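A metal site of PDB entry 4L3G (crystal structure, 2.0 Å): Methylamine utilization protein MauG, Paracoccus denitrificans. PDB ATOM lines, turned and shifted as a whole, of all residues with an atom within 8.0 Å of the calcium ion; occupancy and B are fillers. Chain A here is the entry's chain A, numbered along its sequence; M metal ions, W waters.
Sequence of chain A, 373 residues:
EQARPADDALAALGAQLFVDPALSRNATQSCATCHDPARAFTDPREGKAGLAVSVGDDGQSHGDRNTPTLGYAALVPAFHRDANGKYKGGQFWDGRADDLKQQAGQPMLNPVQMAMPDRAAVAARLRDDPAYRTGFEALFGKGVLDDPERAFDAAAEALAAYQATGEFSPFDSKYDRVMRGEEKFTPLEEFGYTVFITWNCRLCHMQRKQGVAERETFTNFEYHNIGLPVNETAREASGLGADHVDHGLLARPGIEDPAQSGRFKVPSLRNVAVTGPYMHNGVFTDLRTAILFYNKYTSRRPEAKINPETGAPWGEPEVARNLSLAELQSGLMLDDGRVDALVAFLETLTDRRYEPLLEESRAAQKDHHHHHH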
ATOM      1  N   ARG A  39     -13.735  26.554  10.442  1.00  0.00           N
ATOM      2  CA  ARG A  39     -12.442  26.928   9.915  1.00  0.00           C
ATOM      3  C   ARG A  39     -12.276  26.671   8.407  1.00  0.00           C
ATOM      4  O   ARG A  39     -11.286  26.168   7.960  1.00  0.00           O
ATOM      5  CB  ARG A  39     -11.333  26.269  10.695  1.00  0.00           C
ATOM      6  CG  ARG A  39     -10.025  26.966  10.592  1.00  0.00           C
ATOM      7  CD  ARG A  39      -8.913  26.069  11.045  1.00  0.00           C
ATOM      8  NE  ARG A  39      -7.733  26.821  11.336  1.00  0.00           N
ATOM      9  CZ  ARG A  39      -6.668  26.849  10.572  1.00  0.00           C
ATOM     10  NH1 ARG A  39      -5.645  27.600  10.930  1.00  0.00           N
ATOM     11  NH2 ARG A  39      -6.619  26.155   9.463  1.00  0.00           N
ATOM     12  N   THR A  42     -11.153  23.134   7.286  1.00  0.00           N
ATOM     13  CA  THR A  42      -9.792  22.716   7.562  1.00  0.00           C
ATOM     14  C   THR A  42      -9.703  22.332   9.044  1.00  0.00           C
ATOM     15  O   THR A  42     -10.648  22.469   9.773  1.00  0.00           O
ATOM     16  CB  THR A  42      -8.799  23.829   7.210  1.00  0.00           C
ATOM     17  OG1 THR A  42      -8.968  24.975   8.109  1.00  0.00           O
ATOM     18  CG2 THR A  42      -8.971  24.233   5.780  1.00  0.00           C
ATOM     19  N   ASP A  43      -8.550  21.843   9.465  1.00  0.00           N
ATOM     20  CA  ASP A  43      -8.346  21.298  10.804  1.00  0.00           C
ATOM     21  C   ASP A  43      -7.729  22.340  11.809  1.00  0.00           C
ATOM     22  O   ASP A  43      -6.527  22.691  11.718  1.00  0.00           O
ATOM     23  CB  ASP A  43      -7.398  20.133  10.708  1.00  0.00           C
ATOM     24  CG  ASP A  43      -7.347  19.292  11.987  1.00  0.00           C
ATOM     25  OD1 ASP A  43      -7.828  19.744  13.096  1.00  0.00           O
ATOM     26  OD2 ASP A  43      -6.780  18.181  11.862  1.00  0.00           O
ATOM     27  N   LEU A  51      -0.247  22.650  13.178  1.00  0.00           N
ATOM     28  CA  LEU A  51      -1.426  22.430  12.347  1.00  0.00           C
ATOM     29  C   LEU A  51      -1.036  21.929  10.926  1.00  0.00           C
ATOM     30  O   LEU A  51      -1.894  21.899  10.012  1.00  0.00           O
ATOM     31  CB  LEU A  51      -2.241  23.712  12.239  1.00  0.00           C
ATOM     32  CG  LEU A  51      -2.919  24.155  13.531  1.00  0.00           C
ATOM     33  CD1 LEU A  51      -2.162  25.308  14.199  1.00  0.00           C
ATOM     34  CD2 LEU A  51      -4.322  24.595  13.236  1.00  0.00           C
ATOM     35  N   ALA A  52       0.226  21.546  10.750  1.00  0.00           N
ATOM     36  CA  ALA A  52       0.740  21.129   9.448  1.00  0.00           C
ATOM     37  C   ALA A  52       0.046  19.876   8.957  1.00  0.00           C
ATOM     38  O   ALA A  52      -0.279  19.809   7.790  1.00  0.00           O
ATOM     39  CB  ALA A  52       2.227  20.896   9.490  1.00  0.00           C
ATOM     40  N   ASN A  66      -1.048  18.367   4.545  1.00  0.00           N
ATOM     41  CA  ASN A  66      -1.938  19.304   5.236  1.00  0.00           C
ATOM     42  C   ASN A  66      -3.348  19.070   4.782  1.00  0.00           C
ATOM     43  O   ASN A  66      -3.613  18.832   3.554  1.00  0.00           O
ATOM     44  CB  ASN A  66      -1.533  20.687   4.770  1.00  0.00           C
ATOM     45  CG  ASN A  66      -2.286  21.799   5.439  1.00  0.00           C
ATOM     46  OD1 ASN A  66      -2.939  22.642   4.785  1.00  0.00           O
ATOM     47  ND2 ASN A  66      -2.190  21.850   6.780  1.00  0.00           N
ATOM     48  N   THR A  67      -4.277  19.195   5.711  1.00  0.00           N
ATOM     49  CA  THR A  67      -5.665  19.045   5.341  1.00  0.00           C
ATOM     50  C   THR A  67      -6.168  20.244   4.528  1.00  0.00           C
ATOM     51  O   THR A  67      -6.137  21.366   5.038  1.00  0.00           O
ATOM     52  CB  THR A  67      -6.548  18.829   6.569  1.00  0.00           C
ATOM     53  OG1 THR A  67      -6.142  17.628   7.196  1.00  0.00           O
ATOM     54  CG2 THR A  67      -7.982  18.740   6.202  1.00  0.00           C
ATOM     55  N   PRO A  68      -6.651  20.032   3.279  1.00  0.00           N
ATOM     56  CA  PRO A  68      -7.159  21.157   2.478  1.00  0.00           C
ATOM     57  C   PRO A  68      -8.627  21.522   2.753  1.00  0.00           C
ATOM     58  O   PRO A  68      -9.429  20.680   3.160  1.00  0.00           O
ATOM     59  CB  PRO A  68      -7.051  20.621   1.018  1.00  0.00           C
ATOM     60  CG  PRO A  68      -7.337  19.168   1.188  1.00  0.00           C
ATOM     61  CD  PRO A  68      -6.593  18.793   2.472  1.00  0.00           C
ATOM     62  N   THR A  69      -8.993  22.784   2.472  1.00  0.00           N
ATOM     63  CA  THR A  69     -10.418  23.206   2.462  1.00  0.00           C
ATOM     64  C   THR A  69     -11.285  22.382   1.511  1.00  0.00           C
ATOM     65  O   THR A  69     -10.869  21.976   0.439  1.00  0.00           O
ATOM     66  CB  THR A  69     -10.587  24.713   2.091  1.00  0.00           C
ATOM     67  OG1 THR A  69     -11.954  25.099   2.244  1.00  0.00           O
ATOM     68  CG2 THR A  69     -10.182  25.031   0.628  1.00  0.00           C
ATOM     69  N   TRP A  93      -4.160  16.442  -3.014  1.00  0.00           N
ATOM     70  CA  TRP A  93      -3.040  17.267  -3.512  1.00  0.00           C
ATOM     71  C   TRP A  93      -2.316  16.645  -4.716  1.00  0.00           C
ATOM     72  O   TRP A  93      -1.618  17.338  -5.452  1.00  0.00           O
ATOM     73  CB  TRP A  93      -2.029  17.479  -2.411  1.00  0.00           C
ATOM     74  CG  TRP A  93      -2.454  18.388  -1.299  1.00  0.00           C
ATOM     75  CD1 TRP A  93      -2.961  18.014  -0.084  1.00  0.00           C
ATOM     76  CD2 TRP A  93      -2.334  19.793  -1.276  1.00  0.00           C
ATOM     77  NE1 TRP A  93      -3.170  19.154   0.711  1.00  0.00           N
ATOM     78  CE2 TRP A  93      -2.773  20.241   0.001  1.00  0.00           C
ATOM     79  CE3 TRP A  93      -1.869  20.730  -2.193  1.00  0.00           C
ATOM     80  CZ2 TRP A  93      -2.766  21.607   0.357  1.00  0.00           C
ATOM     81  CZ3 TRP A  93      -1.875  22.048  -1.816  1.00  0.00           C
ATOM     82  CH2 TRP A  93      -2.332  22.476  -0.543  1.00  0.00           C
ATOM     83  N   PRO A 267      -3.729  24.814  -5.552  1.00  0.00           N
ATOM     84  CA  PRO A 267      -4.857  25.038  -4.659  1.00  0.00           C
ATOM     85  C   PRO A 267      -5.655  26.259  -5.077  1.00  0.00           C
ATOM     86  O   PRO A 267      -5.075  27.147  -5.686  1.00  0.00           O
ATOM     87  CB  PRO A 267      -4.205  25.232  -3.285  1.00  0.00           C
ATOM     88  CG  PRO A 267      -2.856  25.769  -3.618  1.00  0.00           C
ATOM     89  CD  PRO A 267      -2.458  25.159  -4.917  1.00  0.00           C
ATOM     90  N   ASN A 271     -10.449  31.716   0.451  1.00  0.00           N
ATOM     91  CA  ASN A 271     -10.306  31.450   1.906  1.00  0.00           C
ATOM     92  C   ASN A 271      -8.891  31.225   2.379  1.00  0.00           C
ATOM     93  O   ASN A 271      -8.668  30.800   3.480  1.00  0.00           O
ATOM     94  CB  ASN A 271     -11.185  30.262   2.328  1.00  0.00           C
ATOM     95  CG  ASN A 271     -12.627  30.628   2.277  1.00  0.00           C
ATOM     96  OD1 ASN A 271     -13.017  31.787   2.578  1.00  0.00           O
ATOM     97  ND2 ASN A 271     -13.454  29.664   1.975  1.00  0.00           N
ATOM     98  N   VAL A 272      -7.910  31.595   1.559  1.00  0.00           N
ATOM     99  CA  VAL A 272      -6.550  31.218   1.827  1.00  0.00           C
ATOM    100  C   VAL A 272      -6.112  31.911   3.146  1.00  0.00           C
ATOM    101  O   VAL A 272      -5.270  31.389   3.921  1.00  0.00           O
ATOM    102  CB  VAL A 272      -5.629  31.541   0.615  1.00  0.00           C
ATOM    103  CG1 VAL A 272      -5.532  33.023   0.288  1.00  0.00           C
ATOM    104  CG2 VAL A 272      -4.234  31.020   0.861  1.00  0.00           C
ATOM    105  N   VAL A 274      -7.475  32.188   5.888  1.00  0.00           N
ATOM    106  CA  VAL A 274      -7.849  31.565   7.128  1.00  0.00           C
ATOM    107  C   VAL A 274      -7.581  30.060   7.093  1.00  0.00           C
ATOM    108  O   VAL A 274      -8.068  29.361   7.957  1.00  0.00           O
ATOM    109  CB  VAL A 274      -9.340  31.866   7.468  1.00  0.00           C
ATOM    110  CG1 VAL A 274      -9.583  33.360   7.492  1.00  0.00           C
ATOM    111  CG2 VAL A 274     -10.299  31.160   6.485  1.00  0.00           C
ATOM    112  N   THR A 275      -6.816  29.551   6.133  1.00  0.00           N
ATOM    113  CA  THR A 275      -6.599  28.053   6.040  1.00  0.00           C
ATOM    114  C   THR A 275      -5.133  27.674   6.163  1.00  0.00           C
ATOM    115  O   THR A 275      -4.710  26.586   5.762  1.00  0.00           O
ATOM    116  CB  THR A 275      -7.176  27.419   4.782  1.00  0.00           C
ATOM    117  OG1 THR A 275      -6.500  27.938   3.630  1.00  0.00           O
ATOM    118  CG2 THR A 275      -8.640  27.706   4.684  1.00  0.00           C
ATOM    119  N   GLY A 276      -4.398  28.549   6.837  1.00  0.00           N
ATOM    120  CA  GLY A 276      -2.992  28.330   7.252  1.00  0.00           C
ATOM    121  C   GLY A 276      -2.899  27.100   8.078  1.00  0.00           C
ATOM    122  O   GLY A 276      -3.876  26.723   8.626  1.00  0.00           O
ATOM    123  N   PRO A 277      -1.748  26.438   8.158  1.00  0.00           N
ATOM    124  CA  PRO A 277      -0.527  26.634   7.440  1.00  0.00           C
ATOM    125  C   PRO A 277      -0.659  26.215   5.942  1.00  0.00           C
ATOM    126  O   PRO A 277      -1.710  25.701   5.508  1.00  0.00           O
ATOM    127  CB  PRO A 277       0.485  25.802   8.227  1.00  0.00           C
ATOM    128  CG  PRO A 277      -0.315  24.776   8.852  1.00  0.00           C
ATOM    129  CD  PRO A 277      -1.665  25.335   9.094  1.00  0.00           C
ATOM    130  N   TYR A 278       0.383  26.512   5.181  1.00  0.00           N
ATOM    131  CA  TYR A 278       0.279  26.600   3.719  1.00  0.00           C
ATOM    132  C   TYR A 278       1.092  25.512   3.036  1.00  0.00           C
ATOM    133  O   TYR A 278       2.071  24.991   3.585  1.00  0.00           O
ATOM    134  CB  TYR A 278       0.662  28.023   3.253  1.00  0.00           C
ATOM    135  CG  TYR A 278      -0.311  28.971   3.837  1.00  0.00           C
ATOM    136  CD1 TYR A 278      -1.629  28.968   3.411  1.00  0.00           C
ATOM    137  CD2 TYR A 278       0.055  29.883   4.877  1.00  0.00           C
ATOM    138  CE1 TYR A 278      -2.552  29.791   3.952  1.00  0.00           C
ATOM    139  CE2 TYR A 278      -0.905  30.705   5.459  1.00  0.00           C
ATOM    140  CZ  TYR A 278      -2.192  30.658   5.006  1.00  0.00           C
ATOM    141  OH  TYR A 278      -3.154  31.479   5.534  1.00  0.00           O
ATOM    142  N   MET A 279       0.667  25.235   1.811  1.00  0.00           N
ATOM    143  CA  MET A 279       1.289  24.246   0.967  1.00  0.00           C
ATOM    144  C   MET A 279       0.870  22.819   1.352  1.00  0.00           C
ATOM    145  O   MET A 279       0.358  22.556   2.416  1.00  0.00           O
ATOM    146  CB  MET A 279       2.787  24.440   0.903  1.00  0.00           C
ATOM    147  CG  MET A 279       3.250  25.881   0.546  1.00  0.00           C
ATOM    148  SD  MET A 279       2.605  26.477  -1.049  1.00  0.00           S
ATOM    149  CE  MET A 279       3.281  28.138  -1.121  1.00  0.00           C
ATOM    150  N   HIS A 280       1.120  21.888   0.442  1.00  0.00           N
ATOM    151  CA  HIS A 280       0.738  20.504   0.611  1.00  0.00           C
ATOM    152  C   HIS A 280       1.184  19.849   1.911  1.00  0.00           C
ATOM    153  O   HIS A 280       0.533  18.927   2.394  1.00  0.00           O
ATOM    154  CB  HIS A 280       1.238  19.720  -0.581  1.00  0.00           C
ATOM    155  CG  HIS A 280       2.709  19.468  -0.571  1.00  0.00           C
ATOM    156  ND1 HIS A 280       3.589  20.150  -1.386  1.00  0.00           N
ATOM    157  CD2 HIS A 280       3.449  18.561   0.110  1.00  0.00           C
ATOM    158  CE1 HIS A 280       4.811  19.686  -1.188  1.00  0.00           C
ATOM    159  NE2 HIS A 280       4.752  18.719  -0.298  1.00  0.00           N
ATOM    160  N   ASN A 281       2.304  20.340   2.480  1.00  0.00           N
ATOM    161  CA  ASN A 281       2.858  19.833   3.737  1.00  0.00           C
ATOM    162  C   ASN A 281       2.801  20.860   4.911  1.00  0.00           C
ATOM    163  O   ASN A 281       3.422  20.649   5.938  1.00  0.00           O
ATOM    164  CB  ASN A 281       4.310  19.407   3.521  1.00  0.00           C
ATOM    165  CG  ASN A 281       5.197  20.569   3.092  1.00  0.00           C
ATOM    166  OD1 ASN A 281       4.777  21.722   3.132  1.00  0.00           O
ATOM    167  ND2 ASN A 281       6.402  20.273   2.651  1.00  0.00           N
ATOM    168  N   GLY A 282       2.052  21.928   4.737  1.00  0.00           N
ATOM    169  CA  GLY A 282       1.773  22.852   5.828  1.00  0.00           C
ATOM    170  C   GLY A 282       3.040  23.498   6.322  1.00  0.00           C
ATOM    171  O   GLY A 282       3.127  23.842   7.461  1.00  0.00           O
ATOM    172  N   VAL A 283       4.042  23.624   5.464  1.00  0.00           N
ATOM    173  CA  VAL A 283       5.356  24.061   5.907  1.00  0.00           C
ATOM    174  C   VAL A 283       5.420  25.508   6.420  1.00  0.00           C
ATOM    175  O   VAL A 283       6.245  25.791   7.244  1.00  0.00           O
ATOM    176  CB  VAL A 283       6.402  23.864   4.797  1.00  0.00           C
ATOM    177  CG1 VAL A 283       6.054  24.666   3.527  1.00  0.00           C
ATOM    178  CG2 VAL A 283       7.794  24.159   5.340  1.00  0.00           C
ATOM    179  N   PHE A 284       4.546  26.385   5.933  1.00  0.00           N
ATOM    180  CA  PHE A 284       4.610  27.803   6.308  1.00  0.00           C
ATOM    181  C   PHE A 284       3.376  28.163   7.115  1.00  0.00           C
ATOM    182  O   PHE A 284       2.246  28.055   6.623  1.00  0.00           O
ATOM    183  CB  PHE A 284       4.654  28.697   5.060  1.00  0.00           C
ATOM    184  CG  PHE A 284       5.734  28.360   4.050  1.00  0.00           C
ATOM    185  CD1 PHE A 284       6.981  28.011   4.441  1.00  0.00           C
ATOM    186  CD2 PHE A 284       5.467  28.418   2.696  1.00  0.00           C
ATOM    187  CE1 PHE A 284       7.977  27.718   3.529  1.00  0.00           C
ATOM    188  CE2 PHE A 284       6.448  28.153   1.752  1.00  0.00           C
ATOM    189  CZ  PHE A 284       7.720  27.797   2.168  1.00  0.00           C
HETATM  190 CA    CA M   1      -3.678  24.828   4.649  1.00  0.00          CA
HETATM  191  O   HOH W   1      -2.352  24.369   2.591  1.00  0.00           O
HETATM  192  O   HOH W   2      -5.687  24.001   4.453  1.00  0.00           O
HETATM  193  O   HOH W   3      -4.263  24.208   7.239  1.00  0.00           O
HETATM  194  O   HOH W   4      -4.287  26.378   3.079  1.00  0.00           O
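The backbone NH (N) of Asn 66 lies within hydrogen-bond range of the backbone carbonyl oxygen (O) of His 280.
The backbone carbonyl oxygen of Leu 51 lies within hydrogen-bond range of the side-chain amide nitrogen of Asn 66, 3.2 Å away.
The backbone carbonyl oxygen of Asn 66 lies within hydrogen-bond range of the indole nitrogen of Trp 93, at 2.9 Å.
The backbone carbonyl oxygen of Ala 52 lies within hydrogen-bond range of the side-chain amide nitrogen of Asn 66 (3.0 Å).
Within 4 Å of the calcium ion: Asn 66, Thr 275 and Pro 277.
Along chain A the residues within 4 Å of the calcium ion span positions 66 to 277.
The calcium ion is bound by water W2 (2.2 Å), water W4 (2.3 Å), OD1 of Asn 66 (2.3 Å), O of Pro 277 (2.3 Å), O of Thr 275 (2.3 Å), water W1 (2.5 Å) and water W3 (2.7 Å).
The calcium ion has seven donor atoms within binding distance.
Water W3 lies within hydrogen-bond range of the backbone carbonyl oxygen of Gly 276 (2.9 Å) and the side-chain amide nitrogen of Asn 66 (3.2 Å).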
